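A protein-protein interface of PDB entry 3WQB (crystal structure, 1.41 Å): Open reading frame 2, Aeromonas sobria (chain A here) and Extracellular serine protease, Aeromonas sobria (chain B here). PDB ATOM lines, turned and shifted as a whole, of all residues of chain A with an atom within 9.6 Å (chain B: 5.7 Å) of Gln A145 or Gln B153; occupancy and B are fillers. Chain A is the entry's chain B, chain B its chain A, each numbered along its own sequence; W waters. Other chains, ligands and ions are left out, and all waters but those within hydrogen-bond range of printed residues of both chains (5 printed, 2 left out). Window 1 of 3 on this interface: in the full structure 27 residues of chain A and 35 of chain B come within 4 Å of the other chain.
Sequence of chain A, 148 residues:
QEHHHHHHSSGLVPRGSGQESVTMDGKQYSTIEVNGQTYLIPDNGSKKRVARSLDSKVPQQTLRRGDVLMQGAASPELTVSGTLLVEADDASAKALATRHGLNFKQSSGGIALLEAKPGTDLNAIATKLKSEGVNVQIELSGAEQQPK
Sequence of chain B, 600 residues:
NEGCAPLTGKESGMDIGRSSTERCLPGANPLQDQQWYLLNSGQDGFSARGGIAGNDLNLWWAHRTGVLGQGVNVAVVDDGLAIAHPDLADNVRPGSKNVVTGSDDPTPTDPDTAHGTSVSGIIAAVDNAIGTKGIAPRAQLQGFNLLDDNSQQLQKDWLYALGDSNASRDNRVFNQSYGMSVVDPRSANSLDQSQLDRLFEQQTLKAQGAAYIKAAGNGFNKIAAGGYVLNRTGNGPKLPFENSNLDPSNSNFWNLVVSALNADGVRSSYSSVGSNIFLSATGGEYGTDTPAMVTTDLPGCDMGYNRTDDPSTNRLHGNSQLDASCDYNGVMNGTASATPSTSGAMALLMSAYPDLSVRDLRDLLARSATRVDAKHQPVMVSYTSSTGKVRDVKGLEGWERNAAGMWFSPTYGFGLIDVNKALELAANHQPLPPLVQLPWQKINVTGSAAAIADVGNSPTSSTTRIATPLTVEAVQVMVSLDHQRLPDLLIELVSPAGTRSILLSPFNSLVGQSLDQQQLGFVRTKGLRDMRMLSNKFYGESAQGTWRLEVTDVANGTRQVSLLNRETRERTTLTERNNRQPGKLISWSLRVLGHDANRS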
ATOM      1  N   GLN A  71     -13.108   3.238 -22.653  1.00  0.00           N
ATOM      2  CA  GLN A  71     -14.334   4.023 -22.444  1.00  0.00           C
ATOM      3  C   GLN A  71     -14.508   4.398 -20.975  1.00  0.00           C
ATOM      4  O   GLN A  71     -15.545   4.103 -20.368  1.00  0.00           O
ATOM      5  CB  GLN A  71     -15.578   3.255 -22.903  1.00  0.00           C
ATOM      6  CG  GLN A  71     -15.325   1.889 -23.520  1.00  0.00           C
ATOM      7  CD  GLN A  71     -16.562   1.005 -23.500  1.00  0.00           C
ATOM      8  OE1 GLN A  71     -16.467  -0.210 -23.315  1.00  0.00           O
ATOM      9  NE2 GLN A  71     -17.729   1.611 -23.693  1.00  0.00           N
ATOM     10  N   PRO A  76     -14.922  -2.537 -20.557  1.00  0.00           N
ATOM     11  CA  PRO A  76     -13.925  -3.345 -21.249  1.00  0.00           C
ATOM     12  C   PRO A  76     -13.180  -2.554 -22.315  1.00  0.00           C
ATOM     13  O   PRO A  76     -13.718  -1.596 -22.879  1.00  0.00           O
ATOM     14  CB  PRO A  76     -14.761  -4.455 -21.902  1.00  0.00           C
ATOM     15  CG  PRO A  76     -16.116  -3.865 -22.048  1.00  0.00           C
ATOM     16  CD  PRO A  76     -16.294  -2.995 -20.850  1.00  0.00           C
ATOM     17  N   GLU A  77     -11.941  -2.964 -22.557  1.00  0.00           N
ATOM     18  CA  GLU A  77     -11.130  -2.472 -23.657  1.00  0.00           C
ATOM     19  C   GLU A  77     -11.818  -2.799 -24.984  1.00  0.00           C
ATOM     20  O   GLU A  77     -12.183  -3.952 -25.229  1.00  0.00           O
ATOM     21  CB  GLU A  77      -9.760  -3.148 -23.582  1.00  0.00           C
ATOM     22  CG  GLU A  77      -8.731  -2.657 -24.554  1.00  0.00           C
ATOM     23  CD  GLU A  77      -7.430  -3.419 -24.423  1.00  0.00           C
ATOM     24  OE1 GLU A  77      -7.308  -4.506 -25.032  1.00  0.00           O
ATOM     25  OE2 GLU A  77      -6.530  -2.932 -23.706  1.00  0.00           O
ATOM     26  N   LEU A  78     -11.996  -1.787 -25.833  1.00  0.00           N
ATOM     27  CA  LEU A  78     -12.618  -1.997 -27.145  1.00  0.00           C
ATOM     28  C   LEU A  78     -11.608  -1.896 -28.282  1.00  0.00           C
ATOM     29  O   LEU A  78     -10.628  -1.155 -28.197  1.00  0.00           O
ATOM     30  CB  LEU A  78     -13.769  -1.013 -27.374  1.00  0.00           C
ATOM     31  CG  LEU A  78     -14.913  -0.997 -26.355  1.00  0.00           C
ATOM     32  CD1 LEU A  78     -15.951   0.034 -26.770  1.00  0.00           C
ATOM     33  CD2 LEU A  78     -15.549  -2.366 -26.194  1.00  0.00           C
ATOM     34  N   THR A  79     -11.860  -2.644 -29.348  1.00  0.00           N
ATOM     35  CA  THR A  79     -10.973  -2.663 -30.503  1.00  0.00           C
ATOM     36  C   THR A  79     -11.739  -2.355 -31.779  1.00  0.00           C
ATOM     37  O   THR A  79     -12.842  -2.849 -31.990  1.00  0.00           O
ATOM     38  CB  THR A  79     -10.241  -4.020 -30.622  1.00  0.00           C
ATOM     39  OG1 THR A  79      -9.499  -4.249 -29.419  1.00  0.00           O
ATOM     40  CG2 THR A  79      -9.271  -4.025 -31.789  1.00  0.00           C
ATOM     41  N   SER A  81     -12.678  -3.188 -35.034  1.00  0.00           N
ATOM     42  CA  SER A  81     -12.647  -4.487 -35.706  1.00  0.00           C
ATOM     43  C   SER A  81     -12.292  -4.396 -37.187  1.00  0.00           C
ATOM     44  O   SER A  81     -11.797  -5.365 -37.767  1.00  0.00           O
ATOM     45  CB  SER A  81     -13.990  -5.206 -35.546  1.00  0.00           C
ATOM     46  OG  SER A  81     -14.991  -4.622 -36.367  1.00  0.00           O
ATOM     47  N   LEU A 113     -22.835  -5.093 -43.332  1.00  0.00           N
ATOM     48  CA  LEU A 113     -21.503  -5.129 -42.754  1.00  0.00           C
ATOM     49  C   LEU A 113     -20.492  -4.948 -43.878  1.00  0.00           C
ATOM     50  O   LEU A 113     -20.442  -5.750 -44.822  1.00  0.00           O
ATOM     51  CB  LEU A 113     -21.261  -6.458 -42.033  1.00  0.00           C
ATOM     52  CG  LEU A 113     -21.877  -6.661 -40.644  1.00  0.00           C
ATOM     53  CD1 LEU A 113     -23.404  -6.658 -40.655  1.00  0.00           C
ATOM     54  CD2 LEU A 113     -21.362  -7.948 -40.038  1.00  0.00           C
ATOM     55  N   GLU A 139     -17.716  -0.621 -35.887  1.00  0.00           N
ATOM     56  CA  GLU A 139     -17.748  -1.697 -34.894  1.00  0.00           C
ATOM     57  C   GLU A 139     -16.568  -1.631 -33.929  1.00  0.00           C
ATOM     58  O   GLU A 139     -15.403  -1.648 -34.340  1.00  0.00           O
ATOM     59  CB  GLU A 139     -17.819  -3.082 -35.532  1.00  0.00           C
ATOM     60  CG  GLU A 139     -17.725  -4.186 -34.480  1.00  0.00           C
ATOM     61  CD  GLU A 139     -17.954  -5.566 -35.029  1.00  0.00           C
ATOM     62  OE1 GLU A 139     -17.320  -5.933 -36.036  1.00  0.00           O
ATOM     63  OE2 GLU A 139     -18.751  -6.298 -34.419  1.00  0.00           O
ATOM     64  N   LEU A 140     -16.895  -1.555 -32.649  1.00  0.00           N
ATOM     65  CA  LEU A 140     -15.911  -1.584 -31.581  1.00  0.00           C
ATOM     66  C   LEU A 140     -16.127  -2.872 -30.800  1.00  0.00           C
ATOM     67  O   LEU A 140     -17.101  -3.003 -30.049  1.00  0.00           O
ATOM     68  CB  LEU A 140     -16.043  -0.348 -30.687  1.00  0.00           C
ATOM     69  CG  LEU A 140     -15.961   1.010 -31.406  1.00  0.00           C
ATOM     70  CD1 LEU A 140     -16.207   2.164 -30.432  1.00  0.00           C
ATOM     71  CD2 LEU A 140     -14.632   1.196 -32.152  1.00  0.00           C
ATOM     72  N   SER A 141     -15.219  -3.821 -31.002  1.00  0.00           N
ATOM     73  CA  SER A 141     -15.357  -5.175 -30.481  1.00  0.00           C
ATOM     74  C   SER A 141     -14.712  -5.312 -29.114  1.00  0.00           C
ATOM     75  O   SER A 141     -13.927  -4.465 -28.697  1.00  0.00           O
ATOM     76  CB  SER A 141     -14.732  -6.176 -31.453  1.00  0.00           C
ATOM     77  OG  SER A 141     -13.322  -6.045 -31.460  1.00  0.00           O
ATOM     78  N   GLY A 142     -15.059  -6.389 -28.416  1.00  0.00           N
ATOM     79  CA  GLY A 142     -14.508  -6.652 -27.097  1.00  0.00           C
ATOM     80  C   GLY A 142     -15.487  -7.400 -26.227  1.00  0.00           C
ATOM     81  O   GLY A 142     -16.576  -7.785 -26.678  1.00  0.00           O
ATOM     82  N   ALA A 143     -15.102  -7.584 -24.972  1.00  0.00           N
ATOM     83  CA  ALA A 143     -15.814  -8.469 -24.060  1.00  0.00           C
ATOM     84  C   ALA A 143     -16.976  -7.767 -23.353  1.00  0.00           C
ATOM     85  O   ALA A 143     -17.010  -7.668 -22.128  1.00  0.00           O
ATOM     86  CB  ALA A 143     -14.830  -9.070 -23.057  1.00  0.00           C
ATOM     87  N   GLU A 144     -17.939  -7.292 -24.136  1.00  0.00           N
ATOM     88  CA  GLU A 144     -19.040  -6.509 -23.588  1.00  0.00           C
ATOM     89  C   GLU A 144     -20.071  -7.390 -22.885  1.00  0.00           C
ATOM     90  O   GLU A 144     -20.497  -7.090 -21.765  1.00  0.00           O
ATOM     91  CB  GLU A 144     -19.665  -5.629 -24.672  1.00  0.00           C
ATOM     92  CG  GLU A 144     -18.693  -4.543 -25.121  1.00  0.00           C
ATOM     93  CD  GLU A 144     -19.261  -3.633 -26.184  1.00  0.00           C
ATOM     94  OE1 GLU A 144     -19.653  -2.501 -25.838  1.00  0.00           O
ATOM     95  OE2 GLU A 144     -19.315  -4.049 -27.362  1.00  0.00           O
ATOM     96  N   GLN A 145     -20.455  -8.484 -23.534  1.00  0.00           N
ATOM     97  CA  GLN A 145     -21.338  -9.447 -22.902  1.00  0.00           C
ATOM     98  C   GLN A 145     -20.555 -10.351 -21.953  1.00  0.00           C
ATOM     99  O   GLN A 145     -19.426 -10.766 -22.257  1.00  0.00           O
ATOM    100  CB  GLN A 145     -22.084 -10.265 -23.953  1.00  0.00           C
ATOM    101  CG  GLN A 145     -22.907  -9.422 -24.927  1.00  0.00           C
ATOM    102  CD  GLN A 145     -23.999  -8.596 -24.254  1.00  0.00           C
ATOM    103  OE1 GLN A 145     -24.536  -8.977 -23.209  1.00  0.00           O
ATOM    104  NE2 GLN A 145     -24.332  -7.463 -24.859  1.00  0.00           N
ATOM    105  N   GLN A 146     -21.158 -10.632 -20.804  1.00  0.00           N
ATOM    106  CA  GLN A 146     -20.504 -11.402 -19.758  1.00  0.00           C
ATOM    107  C   GLN A 146     -21.387 -12.583 -19.370  1.00  0.00           C
ATOM    108  O   GLN A 146     -22.608 -12.441 -19.269  1.00  0.00           O
ATOM    109  CB  GLN A 146     -20.287 -10.542 -18.501  1.00  0.00           C
ATOM    110  CG  GLN A 146     -19.895  -9.078 -18.746  1.00  0.00           C
ATOM    111  CD  GLN A 146     -20.384  -8.122 -17.668  1.00  0.00           C
ATOM    112  OE1 GLN A 146     -21.590  -7.900 -17.498  1.00  0.00           O
ATOM    113  NE2 GLN A 146     -19.441  -7.524 -16.952  1.00  0.00           N
ATOM    114  N   PRO A 147     -20.780 -13.748 -19.120  1.00  0.00           N
ATOM    115  CA  PRO A 147     -21.560 -14.865 -18.587  1.00  0.00           C
ATOM    116  C   PRO A 147     -22.196 -14.513 -17.248  1.00  0.00           C
ATOM    117  O   PRO A 147     -21.558 -13.884 -16.390  1.00  0.00           O
ATOM    118  CB  PRO A 147     -20.521 -15.977 -18.416  1.00  0.00           C
ATOM    119  CG  PRO A 147     -19.386 -15.590 -19.300  1.00  0.00           C
ATOM    120  CD  PRO A 147     -19.370 -14.108 -19.352  1.00  0.00           C
ATOM    121  N   LYS A 148     -23.452 -14.906 -17.071  1.00  0.00           N
ATOM    122  CA  LYS A 148     -24.146 -14.646 -15.817  1.00  0.00           C
ATOM    123  C   LYS A 148     -24.250 -15.917 -14.961  1.00  0.00           C
ATOM    124  O   LYS A 148     -25.214 -16.145 -14.214  1.00  0.00           O
ATOM    125  CB  LYS A 148     -25.505 -13.976 -16.078  1.00  0.00           C
ATOM    126  CG  LYS A 148     -25.361 -12.616 -16.769  1.00  0.00           C
ATOM    127  CD  LYS A 148     -24.565 -11.620 -15.923  1.00  0.00           C
ATOM    128  CE  LYS A 148     -24.311 -10.331 -16.686  1.00  0.00           C
ATOM    129  NZ  LYS A 148     -23.469  -9.401 -15.880  1.00  0.00           N
ATOM    130  OXT LYS A 148     -23.321 -16.753 -14.997  1.00  0.00           O
ATOM    131  N   LEU B 146     -19.552 -17.642 -28.378  1.00  0.00           N
ATOM    132  CA  LEU B 146     -19.413 -16.189 -28.434  1.00  0.00           C
ATOM    133  C   LEU B 146     -18.649 -15.594 -27.253  1.00  0.00           C
ATOM    134  O   LEU B 146     -18.020 -14.547 -27.389  1.00  0.00           O
ATOM    135  CB  LEU B 146     -20.803 -15.536 -28.513  1.00  0.00           C
ATOM    136  CG  LEU B 146     -21.303 -15.197 -29.919  1.00  0.00           C
ATOM    137  CD1 LEU B 146     -20.526 -14.004 -30.490  1.00  0.00           C
ATOM    138  CD2 LEU B 146     -21.264 -16.392 -30.881  1.00  0.00           C
ATOM    139  N   LEU B 147     -18.734 -16.253 -26.096  1.00  0.00           N
ATOM    140  CA  LEU B 147     -18.173 -15.728 -24.843  1.00  0.00           C
ATOM    141  C   LEU B 147     -16.824 -16.340 -24.486  1.00  0.00           C
ATOM    142  O   LEU B 147     -16.312 -16.106 -23.391  1.00  0.00           O
ATOM    143  CB  LEU B 147     -19.157 -15.923 -23.686  1.00  0.00           C
ATOM    144  CG  LEU B 147     -20.603 -15.460 -23.882  1.00  0.00           C
ATOM    145  CD1 LEU B 147     -21.438 -15.776 -22.657  1.00  0.00           C
ATOM    146  CD2 LEU B 147     -20.678 -13.992 -24.227  1.00  0.00           C
ATOM    147  N   SER B 151     -12.819 -14.739 -28.025  1.00  0.00           N
ATOM    148  CA  SER B 151     -13.812 -14.193 -28.937  1.00  0.00           C
ATOM    149  C   SER B 151     -13.929 -12.685 -28.734  1.00  0.00           C
ATOM    150  O   SER B 151     -14.054 -12.208 -27.596  1.00  0.00           O
ATOM    151  CB  SER B 151     -15.156 -14.850 -28.694  1.00  0.00           C
ATOM    152  OG  SER B 151     -16.177 -14.143 -29.376  1.00  0.00           O
ATOM    153  N   GLN B 152     -13.888 -11.941 -29.835  1.00  0.00           N
ATOM    154  CA  GLN B 152     -14.067 -10.492 -29.801  1.00  0.00           C
ATOM    155  C   GLN B 152     -15.539 -10.068 -29.816  1.00  0.00           C
ATOM    156  O   GLN B 152     -15.845  -8.874 -29.869  1.00  0.00           O
ATOM    157  CB  GLN B 152     -13.310  -9.828 -30.960  1.00  0.00           C
ATOM    158  CG  GLN B 152     -11.820  -9.653 -30.695  1.00  0.00           C
ATOM    159  CD  GLN B 152     -11.558  -8.762 -29.497  1.00  0.00           C
ATOM    160  OE1 GLN B 152     -11.892  -7.571 -29.491  1.00  0.00           O
ATOM    161  NE2 GLN B 152     -10.980  -9.342 -28.466  1.00  0.00           N
ATOM    162  N   GLN B 153     -16.442 -11.049 -29.765  1.00  0.00           N
ATOM    163  CA  GLN B 153     -17.885 -10.795 -29.783  1.00  0.00           C
ATOM    164  C   GLN B 153     -18.276  -9.932 -30.987  1.00  0.00           C
ATOM    165  O   GLN B 153     -18.934  -8.887 -30.861  1.00  0.00           O
ATOM    166  CB  GLN B 153     -18.363 -10.216 -28.446  1.00  0.00           C
ATOM    167  CG  GLN B 153     -18.021 -11.107 -27.262  1.00  0.00           C
ATOM    168  CD  GLN B 153     -18.558 -10.591 -25.938  1.00  0.00           C
ATOM    169  OE1 GLN B 153     -19.394  -9.679 -25.892  1.00  0.00           O
ATOM    170  NE2 GLN B 153     -18.088 -11.182 -24.849  1.00  0.00           N
ATOM    171  N   LEU B 154     -17.868 -10.404 -32.159  1.00  0.00           N
ATOM    172  CA  LEU B 154     -18.119  -9.722 -33.417  1.00  0.00           C
ATOM    173  C   LEU B 154     -19.570  -9.825 -33.839  1.00  0.00           C
ATOM    174  O   LEU B 154     -20.220 -10.859 -33.649  1.00  0.00           O
ATOM    175  CB  LEU B 154     -17.234 -10.312 -34.518  1.00  0.00           C
ATOM    176  CG  LEU B 154     -15.725 -10.193 -34.292  1.00  0.00           C
ATOM    177  CD1 LEU B 154     -14.969 -10.904 -35.390  1.00  0.00           C
ATOM    178  CD2 LEU B 154     -15.308  -8.735 -34.211  1.00  0.00           C
ATOM    179  N   GLN B 155     -20.064  -8.737 -34.417  1.00  0.00           N
ATOM    180  CA  GLN B 155     -21.418  -8.714 -34.962  1.00  0.00           C
ATOM    181  C   GLN B 155     -21.702  -9.904 -35.885  1.00  0.00           C
ATOM    182  O   GLN B 155     -22.764 -10.519 -35.793  1.00  0.00           O
ATOM    183  CB  GLN B 155     -21.702  -7.395 -35.690  1.00  0.00           C
ATOM    184  CG  GLN B 155     -23.194  -7.188 -36.028  1.00  0.00           C
ATOM    185  CD  GLN B 155     -24.043  -6.847 -34.823  1.00  0.00           C
ATOM    186  OE1 GLN B 155     -23.532  -6.706 -33.714  1.00  0.00           O
ATOM    187  NE2 GLN B 155     -25.348  -6.678 -35.037  1.00  0.00           N
ATOM    188  N   ASP B 157     -20.570 -12.814 -35.776  1.00  0.00           N
ATOM    189  CA  ASP B 157     -20.714 -14.019 -34.962  1.00  0.00           C
ATOM    190  C   ASP B 157     -22.013 -14.019 -34.145  1.00  0.00           C
ATOM    191  O   ASP B 157     -22.648 -15.075 -33.995  1.00  0.00           O
ATOM    192  CB  ASP B 157     -19.485 -14.218 -34.081  1.00  0.00           C
ATOM    193  CG  ASP B 157     -18.232 -14.481 -34.897  1.00  0.00           C
ATOM    194  OD1 ASP B 157     -18.347 -15.087 -35.989  1.00  0.00           O
ATOM    195  OD2 ASP B 157     -17.144 -14.102 -34.433  1.00  0.00           O
ATOM    196  N   TRP B 158     -22.425 -12.850 -33.643  1.00  0.00           N
ATOM    197  CA  TRP B 158     -23.747 -12.753 -33.000  1.00  0.00           C
ATOM    198  C   TRP B 158     -24.851 -13.152 -33.988  1.00  0.00           C
ATOM    199  O   TRP B 158     -25.714 -13.955 -33.663  1.00  0.00           O
ATOM    200  CB  TRP B 158     -24.025 -11.352 -32.439  1.00  0.00           C
ATOM    201  CG  TRP B 158     -23.197 -10.971 -31.245  1.00  0.00           C
ATOM    202  CD1 TRP B 158     -22.291  -9.950 -31.172  1.00  0.00           C
ATOM    203  CD2 TRP B 158     -23.211 -11.586 -29.949  1.00  0.00           C
ATOM    204  NE1 TRP B 158     -21.744  -9.883 -29.909  1.00  0.00           N
ATOM    205  CE2 TRP B 158     -22.279 -10.885 -29.144  1.00  0.00           C
ATOM    206  CE3 TRP B 158     -23.914 -12.663 -29.386  1.00  0.00           C
ATOM    207  CZ2 TRP B 158     -22.030 -11.226 -27.812  1.00  0.00           C
ATOM    208  CZ3 TRP B 158     -23.656 -13.010 -28.062  1.00  0.00           C
ATOM    209  CH2 TRP B 158     -22.729 -12.288 -27.287  1.00  0.00           C
ATOM    210  N   TYR B 178     -26.260 -14.652 -20.574  1.00  0.00           N
ATOM    211  CA  TYR B 178     -25.282 -13.570 -20.536  1.00  0.00           C
ATOM    212  C   TYR B 178     -25.960 -12.208 -20.482  1.00  0.00           C
ATOM    213  O   TYR B 178     -27.170 -12.101 -20.670  1.00  0.00           O
ATOM    214  CB  TYR B 178     -24.307 -13.658 -21.730  1.00  0.00           C
ATOM    215  CG  TYR B 178     -24.965 -13.623 -23.092  1.00  0.00           C
ATOM    216  CD1 TYR B 178     -25.445 -12.420 -23.637  1.00  0.00           C
ATOM    217  CD2 TYR B 178     -25.068 -14.783 -23.860  1.00  0.00           C
ATOM    218  CE1 TYR B 178     -26.042 -12.382 -24.897  1.00  0.00           C
ATOM    219  CE2 TYR B 178     -25.657 -14.757 -25.120  1.00  0.00           C
ATOM    220  CZ  TYR B 178     -26.140 -13.555 -25.631  1.00  0.00           C
ATOM    221  OH  TYR B 178     -26.724 -13.523 -26.873  1.00  0.00           O
ATOM    222  N   GLY B 179     -25.169 -11.174 -20.194  1.00  0.00           N
ATOM    223  CA  GLY B 179     -25.691  -9.826 -20.148  1.00  0.00           C
ATOM    224  C   GLY B 179     -24.573  -8.822 -19.993  1.00  0.00           C
ATOM    225  O   GLY B 179     -23.396  -9.189 -19.854  1.00  0.00           O
ATOM    226  N   MET B 180     -24.959  -7.553 -20.003  1.00  0.00           N
ATOM    227  CA  MET B 180     -24.010  -6.462 -19.925  1.00  0.00           C
ATOM    228  C   MET B 180     -24.313  -5.581 -18.721  1.00  0.00           C
ATOM    229  O   MET B 180     -25.370  -4.958 -18.656  1.00  0.00           O
ATOM    230  CB  MET B 180     -24.047  -5.644 -21.217  1.00  0.00           C
ATOM    231  CG  MET B 180     -22.923  -4.610 -21.291  1.00  0.00           C
ATOM    232  SD  MET B 180     -22.950  -3.685 -22.822  1.00  0.00           S
ATOM    233  CE  MET B 180     -24.447  -2.791 -22.576  1.00  0.00           C
ATOM    234  N   LYS B 214     -33.316 -14.950 -21.834  1.00  0.00           N
ATOM    235  CA  LYS B 214     -32.272 -14.001 -21.510  1.00  0.00           C
ATOM    236  C   LYS B 214     -32.068 -13.842 -20.002  1.00  0.00           C
ATOM    237  O   LYS B 214     -33.024 -13.601 -19.262  1.00  0.00           O
ATOM    238  CB  LYS B 214     -32.634 -12.651 -22.139  1.00  0.00           C
ATOM    239  CG  LYS B 214     -31.626 -11.525 -21.932  1.00  0.00           C
ATOM    240  CD  LYS B 214     -30.274 -11.838 -22.577  1.00  0.00           C
ATOM    241  CE  LYS B 214     -29.426 -10.593 -22.703  1.00  0.00           C
ATOM    242  NZ  LYS B 214     -29.021 -10.056 -21.363  1.00  0.00           N
ATOM    243  N   ASP B 247     -29.459  -3.001 -18.863  1.00  0.00           N
ATOM    244  CA  ASP B 247     -28.862  -3.564 -20.071  1.00  0.00           C
ATOM    245  C   ASP B 247     -29.869  -3.372 -21.205  1.00  0.00           C
ATOM    246  O   ASP B 247     -30.969  -3.922 -21.137  1.00  0.00           O
ATOM    247  CB  ASP B 247     -28.537  -5.047 -19.851  1.00  0.00           C
ATOM    248  CG  ASP B 247     -28.060  -5.758 -21.117  1.00  0.00           C
ATOM    249  OD1 ASP B 247     -28.125  -5.184 -22.234  1.00  0.00           O
ATOM    250  OD2 ASP B 247     -27.615  -6.917 -20.975  1.00  0.00           O
ATOM    251  N   SER B 249     -30.437  -4.560 -24.079  1.00  0.00           N
ATOM    252  CA  SER B 249     -31.001  -5.741 -24.732  1.00  0.00           C
ATOM    253  C   SER B 249     -32.177  -6.329 -23.957  1.00  0.00           C
ATOM    254  O   SER B 249     -33.044  -6.991 -24.531  1.00  0.00           O
ATOM    255  CB  SER B 249     -29.931  -6.810 -24.912  1.00  0.00           C
ATOM    256  OG  SER B 249     -28.876  -6.308 -25.704  1.00  0.00           O
HETATM  257  O   HOH W   1     -26.525  -5.453 -24.448  1.00  0.00           O
HETATM  258  O   HOH W   2     -18.613  -6.201 -31.666  1.00  0.00           O
HETATM  259  O   HOH W   3     -18.582  -8.268 -37.246  1.00  0.00           O
HETATM  260  O   HOH W   4     -27.144  -8.439 -23.018  1.00  0.00           O
HETATM  261  O   HOH W   5     -21.132  -4.963 -33.255  1.00  0.00           O
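Of the printed residues of chain B, Ser A141 touches Gln B152 (2.9 Å) and Leu B154 (3.8 Å).
Of the printed residues of chain B, Gly A142 touches Gln B152 (3.0 Å) and Gln B153 (3.5 Å).
Printed residues of chain B within 4 Å of Gln A145: Leu B147 (3.98 Å), Gln B153 (2.8 Å), Trp B158 (3.5 Å), Tyr B178 (3.6 Å), Gly B179 (3.2 Å) and Met B180 (3.5 Å).
Of the printed residues of chain B, Pro A147 touches Leu B147.
No residue of chain A comes within 4 Å of Ser B151.
Of chain A, only Gly A142 (3.5 Å), Ala A143 (3.6 Å), Glu A144 (3.3 Å) and Gln A145 (2.8 Å) come within 4 Å of Gln B153.
Of the printed residues of chain A, Tyr B178 touches Gln A145 (3.6 Å), Gln A146 (3.2 Å) and Lys A148 (3.8 Å).
Gly B179 touches three residues of chain A.
Ser B249 touches none of the printed residues of chain A.
The nearest printed residue of chain B that does not touch Gln A145 is Asp B247 (4.3 Å).
The nearest residue of chain A that does not touch Gln B153 is Glu A139 (4.4 Å).
The backbone carbonyl oxygen (O) of Gln B153 sits at hydrogen-bond distance from the indole nitrogen (NE1) of Trp B158, 3.1 Å away.
The backbone carbonyl oxygen of Tyr B178 is in hydrogen-bond range of the side-chain amino group of Lys B214 (2.8 Å).
N of Met B180 is in hydrogen-bond range of OD2 of Asp B247.
N of Ser A141 is in hydrogen-bond range of O of Thr A79 (2.8 Å).
OE1 of Glu A139 is in hydrogen-bond range of OG of Ser A81 (2.7 Å).
OE1 of Gln A146 lies within hydrogen-bond range of NZ of Lys A148 (2.9 Å).
Hydrophobic or aromatic side chains of chain B that line the printed part of chain A: Leu B147, Leu B154, Trp B158, Tyr B178 and Met B180.
Along chain B the printed residues that touch a printed residue of chain A span positions 147 to 180.
Of the 17 printed residues of chain A, 10 touch a printed residue of chain B.
Among the printed residues, merely in contact across the chains: Gln A146 with Tyr B178 (3.2 Å), Gln A145 with Gly B179 (3.2 Å), Lys A148 with Gly B179 (3.5 Å), Glu A144 with Met B180 (3.5 Å), Gln A145 with Trp B158 (3.5 Å), Gln A145 with Met B180 (3.5 Å), Gln A145 with Tyr B178 (3.6 Å), Glu A139 with Leu B154 (3.6 Å), Ala A143 with Gln B153 (3.6 Å), Gln A146 with Met B180 (3.7 Å), Lys A148 with Tyr B178 (3.8 Å), Ser A141 with Leu B154 (3.8 Å), Pro A147 with Leu B147 (3.9 Å), Gln A145 with Leu B147 (3.98 Å) and Ser A81 with Leu B154 (3.997 Å).
The side-chain amide oxygen (OE1) of Gln B152 sits at hydrogen-bond distance from the side-chain hydroxyl (OG) of Ser A141, 2.9 Å away.
The backbone carbonyl oxygen (O) of Gln B152 sits at hydrogen-bond distance from the backbone NH (N) of Gly A142 (3.0 Å).
OE1 of Gln B153 sits close to O of Gly A142 (3.5 Å).
The backbone NH (N) of Glu A144 sits at hydrogen-bond distance from the side-chain amide oxygen (OE1) of Gln B153.
N of Gln A145 sits at hydrogen-bond distance from OE1 of Gln B153 (2.8 Å).
OE2 of Glu A139 lies within hydrogen-bond range of N of Gln B155 (2.8 Å).
The backbone carbonyl oxygen of Gly B179 lies within hydrogen-bond range of the backbone NH of Gln A146 (2.8 Å).
Water W4 lies within hydrogen-bond range of the side-chain carboxylate of Asp B247 (2.6 Å), the side-chain amide oxygen of Gln A145 (2.7 Å) and the side-chain amino group of Lys B214 (3.0 Å).
Water W1 lies within hydrogen-bond range of the side-chain carboxylate (OD1) of Asp B247 (2.7 Å), the side-chain hydroxyl (OG) of Ser B249 (2.8 Å) and the side-chain amide nitrogen (NE2) of Gln A145 (3.0 Å).
Water W2 lies within hydrogen-bond range of OE2 of Glu A139 (2.8 Å) and O of Gln B153 (2.8 Å).
Water W3 bridges the side-chain carboxylate of Glu A139 (2.9 Å) and the backbone NH of Gln B155 (3.2 Å).
Water W5 lies within hydrogen-bond range of OE2 of Glu A139 (3.0 Å) and OE1 of Gln B155 (3.0 Å).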
